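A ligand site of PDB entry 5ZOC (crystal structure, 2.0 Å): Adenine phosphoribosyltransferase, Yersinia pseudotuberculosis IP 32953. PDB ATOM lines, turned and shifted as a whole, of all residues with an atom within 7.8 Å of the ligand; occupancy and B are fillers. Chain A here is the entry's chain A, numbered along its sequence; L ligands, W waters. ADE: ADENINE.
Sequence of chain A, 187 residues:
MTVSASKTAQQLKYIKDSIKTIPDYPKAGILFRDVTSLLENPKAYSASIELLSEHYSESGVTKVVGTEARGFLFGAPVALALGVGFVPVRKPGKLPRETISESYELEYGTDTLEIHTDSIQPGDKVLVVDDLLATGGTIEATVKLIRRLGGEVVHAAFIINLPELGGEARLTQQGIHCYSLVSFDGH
The chain-end carboxylate of His 187 lies within hydrogen-bond range of a nitrogen (N7) of the ligand, at 2.8 Å.
O of Leu 31 is in hydrogen-bond range of N6 of the ligand (3.1 Å).
A nitrogen (N1) of the ligand lies within hydrogen-bond range of the backbone NH (N) of Arg 33 (3.1 Å).
NE of Arg 33 is in hydrogen-bond range of O of Leu 31, 3.2 Å away.
NH1 of Arg 33 sits at hydrogen-bond distance from O of Asp 185 (3.0 Å).
OG1 of Thr 21 is in hydrogen-bond range of NH2 of Arg 33 (2.9 Å).
O of Phe 32 lies within hydrogen-bond range of N of Ile 22 (2.7 Å).
The backbone carbonyl oxygen (O) of Leu 133 lies within hydrogen-bond range of the backbone NH (N) of Leu 162, 3.0 Å away.
Ile 30 touches the ligand (CG2 to N6, 3.9 Å).
Phe 32 touches the ligand.
Leu 132 touches the ligand.
Leu 162 touches the ligand (CD1 to C5, 3.5 Å).
Leu 165 touches the ligand (CD1 to C8, 3.9 Å).
Hydrophobic or aromatic side chains within 4 Å of the ligand: Ile 30, Phe 32, Leu 132, Leu 162 and Leu 165.
Within 4 Å of the ligand: Ile 30, Leu 31, Phe 32, Arg 33, Leu 132, Leu 162, Leu 165 and His 187.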
ATOM      1  N   LYS A  20     -10.181   7.524  28.982  1.00  0.00           N
ATOM      2  CA  LYS A  20     -10.995   8.108  30.070  1.00  0.00           C
ATOM      3  C   LYS A  20     -12.463   8.242  29.675  1.00  0.00           C
ATOM      4  O   LYS A  20     -12.779   8.330  28.496  1.00  0.00           O
ATOM      5  CB  LYS A  20     -10.438   9.472  30.454  1.00  0.00           C
ATOM      6  CG  LYS A  20      -9.197   9.400  31.313  1.00  0.00           C
ATOM      7  CD  LYS A  20      -8.452  10.723  31.278  1.00  0.00           C
ATOM      8  CE  LYS A  20      -7.317  10.747  32.283  1.00  0.00           C
ATOM      9  NZ  LYS A  20      -7.850  10.725  33.662  1.00  0.00           N
ATOM     10  N   THR A  21     -13.360   8.281  30.661  1.00  0.00           N
ATOM     11  CA  THR A  21     -14.784   8.511  30.414  1.00  0.00           C
ATOM     12  C   THR A  21     -15.212   9.779  31.123  1.00  0.00           C
ATOM     13  O   THR A  21     -14.903   9.978  32.282  1.00  0.00           O
ATOM     14  CB  THR A  21     -15.657   7.343  30.905  1.00  0.00           C
ATOM     15  OG1 THR A  21     -15.343   6.154  30.162  1.00  0.00           O
ATOM     16  CG2 THR A  21     -17.146   7.661  30.737  1.00  0.00           C
ATOM     17  N   ILE A  22     -15.920  10.654  30.410  1.00  0.00           N
ATOM     18  CA  ILE A  22     -16.399  11.909  30.984  1.00  0.00           C
ATOM     19  C   ILE A  22     -17.925  11.895  30.964  1.00  0.00           C
ATOM     20  O   ILE A  22     -18.537  11.958  29.912  1.00  0.00           O
ATOM     21  CB  ILE A  22     -15.915  13.133  30.167  1.00  0.00           C
ATOM     22  CG1 ILE A  22     -14.401  13.292  30.265  1.00  0.00           C
ATOM     23  CG2 ILE A  22     -16.570  14.411  30.683  1.00  0.00           C
ATOM     24  CD1 ILE A  22     -13.617  12.333  29.404  1.00  0.00           C
ATOM     25  N   TYR A  25     -21.260  14.558  29.330  1.00  0.00           N
ATOM     26  CA  TYR A  25     -20.716  15.357  28.259  1.00  0.00           C
ATOM     27  C   TYR A  25     -20.950  14.558  26.981  1.00  0.00           C
ATOM     28  O   TYR A  25     -20.748  13.340  26.979  1.00  0.00           O
ATOM     29  CB  TYR A  25     -19.226  15.596  28.498  1.00  0.00           C
ATOM     30  CG  TYR A  25     -18.523  16.307  27.367  1.00  0.00           C
ATOM     31  CD1 TYR A  25     -18.133  15.613  26.240  1.00  0.00           C
ATOM     32  CD2 TYR A  25     -18.256  17.657  27.437  1.00  0.00           C
ATOM     33  CE1 TYR A  25     -17.486  16.259  25.195  1.00  0.00           C
ATOM     34  CE2 TYR A  25     -17.613  18.315  26.398  1.00  0.00           C
ATOM     35  CZ  TYR A  25     -17.234  17.610  25.284  1.00  0.00           C
ATOM     36  OH  TYR A  25     -16.595  18.234  24.244  1.00  0.00           O
ATOM     37  N   PRO A  26     -21.405  15.219  25.906  1.00  0.00           N
ATOM     38  CA  PRO A  26     -21.662  16.657  25.775  1.00  0.00           C
ATOM     39  C   PRO A  26     -23.061  17.080  26.261  1.00  0.00           C
ATOM     40  O   PRO A  26     -23.432  18.242  26.099  1.00  0.00           O
ATOM     41  CB  PRO A  26     -21.524  16.901  24.277  1.00  0.00           C
ATOM     42  CG  PRO A  26     -21.757  15.574  23.614  1.00  0.00           C
ATOM     43  CD  PRO A  26     -21.708  14.498  24.663  1.00  0.00           C
ATOM     44  N   GLY A  29     -26.262  12.135  30.639  1.00  0.00           N
ATOM     45  CA  GLY A  29     -26.569  10.739  30.307  1.00  0.00           C
ATOM     46  C   GLY A  29     -25.573  10.046  29.384  1.00  0.00           C
ATOM     47  O   GLY A  29     -25.468   8.828  29.391  1.00  0.00           O
ATOM     48  N   ILE A  30     -24.856  10.828  28.577  1.00  0.00           N
ATOM     49  CA  ILE A  30     -23.841  10.277  27.678  1.00  0.00           C
ATOM     50  C   ILE A  30     -22.511  10.139  28.420  1.00  0.00           C
ATOM     51  O   ILE A  30     -22.070  11.074  29.098  1.00  0.00           O
ATOM     52  CB  ILE A  30     -23.615  11.184  26.448  1.00  0.00           C
ATOM     53  CG1 ILE A  30     -24.855  11.193  25.552  1.00  0.00           C
ATOM     54  CG2 ILE A  30     -22.410  10.718  25.645  1.00  0.00           C
ATOM     55  CD1 ILE A  30     -25.163   9.858  24.893  1.00  0.00           C
ATOM     56  N   LEU A  31     -21.894   8.960  28.313  1.00  0.00           N
ATOM     57  CA  LEU A  31     -20.574   8.746  28.889  1.00  0.00           C
ATOM     58  C   LEU A  31     -19.517   8.929  27.804  1.00  0.00           C
ATOM     59  O   LEU A  31     -19.252   8.008  27.022  1.00  0.00           O
ATOM     60  CB  LEU A  31     -20.458   7.348  29.494  1.00  0.00           C
ATOM     61  CG  LEU A  31     -21.267   7.071  30.765  1.00  0.00           C
ATOM     62  CD1 LEU A  31     -22.704   6.729  30.425  1.00  0.00           C
ATOM     63  CD2 LEU A  31     -20.644   5.937  31.565  1.00  0.00           C
ATOM     64  N   PHE A  32     -18.903  10.105  27.737  1.00  0.00           N
ATOM     65  CA  PHE A  32     -17.954  10.377  26.647  1.00  0.00           C
ATOM     66  C   PHE A  32     -16.680   9.575  26.818  1.00  0.00           C
ATOM     67  O   PHE A  32     -16.061   9.580  27.886  1.00  0.00           O
ATOM     68  CB  PHE A  32     -17.644  11.867  26.509  1.00  0.00           C
ATOM     69  CG  PHE A  32     -17.054  12.237  25.169  1.00  0.00           C
ATOM     70  CD1 PHE A  32     -17.888  12.515  24.084  1.00  0.00           C
ATOM     71  CD2 PHE A  32     -15.685  12.310  25.006  1.00  0.00           C
ATOM     72  CE1 PHE A  32     -17.344  12.864  22.859  1.00  0.00           C
ATOM     73  CE2 PHE A  32     -15.151  12.648  23.779  1.00  0.00           C
ATOM     74  CZ  PHE A  32     -15.974  12.925  22.703  1.00  0.00           C
ATOM     75  N   ARG A  33     -16.306   8.858  25.767  1.00  0.00           N
ATOM     76  CA  ARG A  33     -15.108   8.052  25.744  1.00  0.00           C
ATOM     77  C   ARG A  33     -14.027   8.873  25.054  1.00  0.00           C
ATOM     78  O   ARG A  33     -14.107   9.124  23.842  1.00  0.00           O
ATOM     79  CB  ARG A  33     -15.352   6.746  24.993  1.00  0.00           C
ATOM     80  CG  ARG A  33     -16.696   6.100  25.346  1.00  0.00           C
ATOM     81  CD  ARG A  33     -16.795   5.701  26.811  1.00  0.00           C
ATOM     82  NE  ARG A  33     -18.084   5.080  27.107  1.00  0.00           N
ATOM     83  CZ  ARG A  33     -18.394   4.471  28.245  1.00  0.00           C
ATOM     84  NH1 ARG A  33     -19.590   3.917  28.396  1.00  0.00           N
ATOM     85  NH2 ARG A  33     -17.518   4.406  29.244  1.00  0.00           N
ATOM     86  N   ASP A  34     -13.015   9.268  25.833  1.00  0.00           N
ATOM     87  CA  ASP A  34     -12.032  10.256  25.432  1.00  0.00           C
ATOM     88  C   ASP A  34     -10.724   9.586  25.068  1.00  0.00           C
ATOM     89  O   ASP A  34      -9.954   9.153  25.936  1.00  0.00           O
ATOM     90  CB  ASP A  34     -11.819  11.253  26.588  1.00  0.00           C
ATOM     91  CG  ASP A  34     -10.684  12.231  26.327  1.00  0.00           C
ATOM     92  OD1 ASP A  34     -10.148  12.270  25.183  1.00  0.00           O
ATOM     93  OD2 ASP A  34     -10.336  12.977  27.270  1.00  0.00           O
ATOM     94  N   VAL A  35     -10.464   9.530  23.774  1.00  0.00           N
ATOM     95  CA  VAL A  35      -9.272   8.861  23.231  1.00  0.00           C
ATOM     96  C   VAL A  35      -7.978   9.691  23.380  1.00  0.00           C
ATOM     97  O   VAL A  35      -6.894   9.167  23.161  1.00  0.00           O
ATOM     98  CB  VAL A  35      -9.503   8.469  21.744  1.00  0.00           C
ATOM     99  CG1 VAL A  35      -9.304   9.650  20.813  1.00  0.00           C
ATOM    100  CG2 VAL A  35      -8.592   7.336  21.354  1.00  0.00           C
ATOM    101  N   ARG A  70      -9.349  13.085  13.704  1.00  0.00           N
ATOM    102  CA  ARG A  70      -8.952  12.016  14.626  1.00  0.00           C
ATOM    103  C   ARG A  70      -8.606  10.759  13.886  1.00  0.00           C
ATOM    104  O   ARG A  70      -7.806   9.955  14.361  1.00  0.00           O
ATOM    105  CB  ARG A  70     -10.069  11.710  15.602  1.00  0.00           C
ATOM    106  CG  ARG A  70     -10.149  12.697  16.729  1.00  0.00           C
ATOM    107  CD  ARG A  70      -9.470  12.150  17.955  1.00  0.00           C
ATOM    108  NE  ARG A  70      -9.616  13.064  19.072  1.00  0.00           N
ATOM    109  CZ  ARG A  70     -10.792  13.394  19.599  1.00  0.00           C
ATOM    110  NH1 ARG A  70     -11.916  12.895  19.090  1.00  0.00           N
ATOM    111  NH2 ARG A  70     -10.843  14.252  20.628  1.00  0.00           N
ATOM    112  N   ASP A 131     -10.897   6.630  14.609  1.00  0.00           N
ATOM    113  CA  ASP A 131     -10.740   6.445  16.038  1.00  0.00           C
ATOM    114  C   ASP A 131     -11.902   5.677  16.668  1.00  0.00           C
ATOM    115  O   ASP A 131     -11.695   4.774  17.482  1.00  0.00           O
ATOM    116  CB  ASP A 131     -10.524   7.790  16.749  1.00  0.00           C
ATOM    117  CG  ASP A 131     -11.711   8.755  16.647  1.00  0.00           C
ATOM    118  OD1 ASP A 131     -12.529   8.654  15.717  1.00  0.00           O
ATOM    119  OD2 ASP A 131     -11.807   9.647  17.507  1.00  0.00           O
ATOM    120  N   LEU A 132     -13.115   6.051  16.336  1.00  0.00           N
ATOM    121  CA  LEU A 132     -14.273   5.536  17.055  1.00  0.00           C
ATOM    122  C   LEU A 132     -15.421   5.296  16.097  1.00  0.00           C
ATOM    123  O   LEU A 132     -15.695   6.121  15.238  1.00  0.00           O
ATOM    124  CB  LEU A 132     -14.663   6.526  18.179  1.00  0.00           C
ATOM    125  CG  LEU A 132     -15.891   6.219  19.041  1.00  0.00           C
ATOM    126  CD1 LEU A 132     -15.671   6.737  20.450  1.00  0.00           C
ATOM    127  CD2 LEU A 132     -17.166   6.806  18.454  1.00  0.00           C
ATOM    128  N   LEU A 133     -16.059   4.144  16.211  1.00  0.00           N
ATOM    129  CA  LEU A 133     -17.203   3.849  15.367  1.00  0.00           C
ATOM    130  C   LEU A 133     -18.487   4.134  16.122  1.00  0.00           C
ATOM    131  O   LEU A 133     -18.820   3.417  17.070  1.00  0.00           O
ATOM    132  CB  LEU A 133     -17.213   2.372  14.900  1.00  0.00           C
ATOM    133  CG  LEU A 133     -18.387   1.965  14.015  1.00  0.00           C
ATOM    134  CD1 LEU A 133     -18.497   2.815  12.757  1.00  0.00           C
ATOM    135  CD2 LEU A 133     -18.272   0.488  13.643  1.00  0.00           C
ATOM    136  N   ALA A 134     -19.206   5.148  15.673  1.00  0.00           N
ATOM    137  CA  ALA A 134     -20.480   5.483  16.258  1.00  0.00           C
ATOM    138  C   ALA A 134     -21.624   5.098  15.292  1.00  0.00           C
ATOM    139  O   ALA A 134     -21.965   3.915  15.186  1.00  0.00           O
ATOM    140  CB  ALA A 134     -20.490   6.970  16.637  1.00  0.00           C
ATOM    141  N   THR A 135     -22.196   6.078  14.583  1.00  0.00           N
ATOM    142  CA  THR A 135     -23.258   5.752  13.613  1.00  0.00           C
ATOM    143  C   THR A 135     -22.704   5.212  12.301  1.00  0.00           C
ATOM    144  O   THR A 135     -23.401   4.485  11.586  1.00  0.00           O
ATOM    145  CB  THR A 135     -24.147   6.966  13.273  1.00  0.00           C
ATOM    146  OG1 THR A 135     -23.337   7.993  12.673  1.00  0.00           O
ATOM    147  CG2 THR A 135     -24.833   7.518  14.526  1.00  0.00           C
ATOM    148  N   ILE A 160     -12.105   2.294  18.986  1.00  0.00           N
ATOM    149  CA  ILE A 160     -13.324   2.092  19.787  1.00  0.00           C
ATOM    150  C   ILE A 160     -14.550   1.825  18.925  1.00  0.00           C
ATOM    151  O   ILE A 160     -14.777   2.503  17.907  1.00  0.00           O
ATOM    152  CB  ILE A 160     -13.617   3.334  20.654  1.00  0.00           C
ATOM    153  CG1 ILE A 160     -12.437   3.664  21.575  1.00  0.00           C
ATOM    154  CG2 ILE A 160     -14.883   3.114  21.478  1.00  0.00           C
ATOM    155  CD1 ILE A 160     -12.549   5.004  22.260  1.00  0.00           C
ATOM    156  N   LEU A 162     -18.756   1.564  19.481  1.00  0.00           N
ATOM    157  CA  LEU A 162     -19.943   1.713  20.318  1.00  0.00           C
ATOM    158  C   LEU A 162     -21.073   0.963  19.627  1.00  0.00           C
ATOM    159  O   LEU A 162     -21.857   1.558  18.866  1.00  0.00           O
ATOM    160  CB  LEU A 162     -20.320   3.180  20.515  1.00  0.00           C
ATOM    161  CG  LEU A 162     -19.205   4.099  21.034  1.00  0.00           C
ATOM    162  CD1 LEU A 162     -19.713   5.532  21.151  1.00  0.00           C
ATOM    163  CD2 LEU A 162     -18.690   3.627  22.383  1.00  0.00           C
ATOM    164  N   LEU A 165     -24.804   2.039  18.681  1.00  0.00           N
ATOM    165  CA  LEU A 165     -25.147   3.102  17.724  1.00  0.00           C
ATOM    166  C   LEU A 165     -25.325   2.568  16.292  1.00  0.00           C
ATOM    167  O   LEU A 165     -25.605   3.349  15.374  1.00  0.00           O
ATOM    168  CB  LEU A 165     -24.104   4.223  17.752  1.00  0.00           C
ATOM    169  CG  LEU A 165     -24.058   4.944  19.098  1.00  0.00           C
ATOM    170  CD1 LEU A 165     -23.012   6.066  19.099  1.00  0.00           C
ATOM    171  CD2 LEU A 165     -25.431   5.483  19.453  1.00  0.00           C
ATOM    172  N   PHE A 184     -17.530  -0.242  23.911  1.00  0.00           N
ATOM    173  CA  PHE A 184     -18.161   0.388  25.072  1.00  0.00           C
ATOM    174  C   PHE A 184     -19.680   0.394  24.918  1.00  0.00           C
ATOM    175  O   PHE A 184     -20.209   0.437  23.812  1.00  0.00           O
ATOM    176  CB  PHE A 184     -17.678   1.837  25.241  1.00  0.00           C
ATOM    177  CG  PHE A 184     -16.286   1.969  25.822  1.00  0.00           C
ATOM    178  CD1 PHE A 184     -16.055   1.736  27.167  1.00  0.00           C
ATOM    179  CD2 PHE A 184     -15.226   2.370  25.033  1.00  0.00           C
ATOM    180  CE1 PHE A 184     -14.785   1.878  27.712  1.00  0.00           C
ATOM    181  CE2 PHE A 184     -13.962   2.519  25.563  1.00  0.00           C
ATOM    182  CZ  PHE A 184     -13.732   2.269  26.907  1.00  0.00           C
ATOM    183  N   ASP A 185     -20.364   0.356  26.058  1.00  0.00           N
ATOM    184  CA  ASP A 185     -21.813   0.460  26.078  1.00  0.00           C
ATOM    185  C   ASP A 185     -22.219   1.920  26.008  1.00  0.00           C
ATOM    186  O   ASP A 185     -21.432   2.815  26.330  1.00  0.00           O
ATOM    187  CB  ASP A 185     -22.372  -0.151  27.356  1.00  0.00           C
ATOM    188  CG  ASP A 185     -22.088  -1.621  27.468  1.00  0.00           C
ATOM    189  OD1 ASP A 185     -22.213  -2.329  26.440  1.00  0.00           O
ATOM    190  OD2 ASP A 185     -21.734  -2.078  28.562  1.00  0.00           O
ATOM    191  N   GLY A 186     -23.446   2.165  25.586  1.00  0.00           N
ATOM    192  CA  GLY A 186     -24.003   3.503  25.596  1.00  0.00           C
ATOM    193  C   GLY A 186     -24.036   4.188  24.252  1.00  0.00           C
ATOM    194  O   GLY A 186     -23.457   3.717  23.272  1.00  0.00           O
ATOM    195  N   HIS A 187     -24.739   5.318  24.227  1.00  0.00           N
ATOM    196  CA  HIS A 187     -24.831   6.152  23.049  1.00  0.00           C
ATOM    197  C   HIS A 187     -23.703   7.194  23.008  1.00  0.00           C
ATOM    198  O   HIS A 187     -22.852   7.222  23.906  1.00  0.00           O
ATOM    199  CB  HIS A 187     -26.212   6.813  23.026  1.00  0.00           C
ATOM    200  CG  HIS A 187     -27.312   5.839  22.771  1.00  0.00           C
ATOM    201  ND1 HIS A 187     -28.569   6.215  22.355  1.00  0.00           N
ATOM    202  CD2 HIS A 187     -27.341   4.484  22.845  1.00  0.00           C
ATOM    203  CE1 HIS A 187     -29.321   5.143  22.199  1.00  0.00           C
ATOM    204  NE2 HIS A 187     -28.601   4.080  22.498  1.00  0.00           N
ATOM    205  OXT HIS A 187     -23.616   7.988  22.080  1.00  0.00           O
HETATM  206  N9  ADE L   1     -19.797   9.767  19.619  1.00  0.00           N
HETATM  207  C8  ADE L   1     -21.050   9.333  19.914  1.00  0.00           C
HETATM  208  N7  ADE L   1     -21.109   8.865  21.184  1.00  0.00           N
HETATM  209  C5  ADE L   1     -19.879   8.977  21.716  1.00  0.00           C
HETATM  210  C6  ADE L   1     -19.255   8.662  23.024  1.00  0.00           C
HETATM  211  N6  ADE L   1     -19.956   8.116  24.042  1.00  0.00           N
HETATM  212  N1  ADE L   1     -17.946   8.961  23.169  1.00  0.00           N
HETATM  213  C2  ADE L   1     -17.215   9.496  22.168  1.00  0.00           C
HETATM  214  N3  ADE L   1     -17.728   9.812  20.975  1.00  0.00           N
HETATM  215  C4  ADE L   1     -19.021   9.573  20.690  1.00  0.00           C
HETATM  216  O   HOH W   1     -16.102  10.843  19.479  1.00  0.00           O
HETATM  217  O   HOH W   2     -18.564  10.323  17.256  1.00  0.00           O
HETATM  218  O   HOH W   3     -20.638   5.442  25.396  1.00  0.00           O
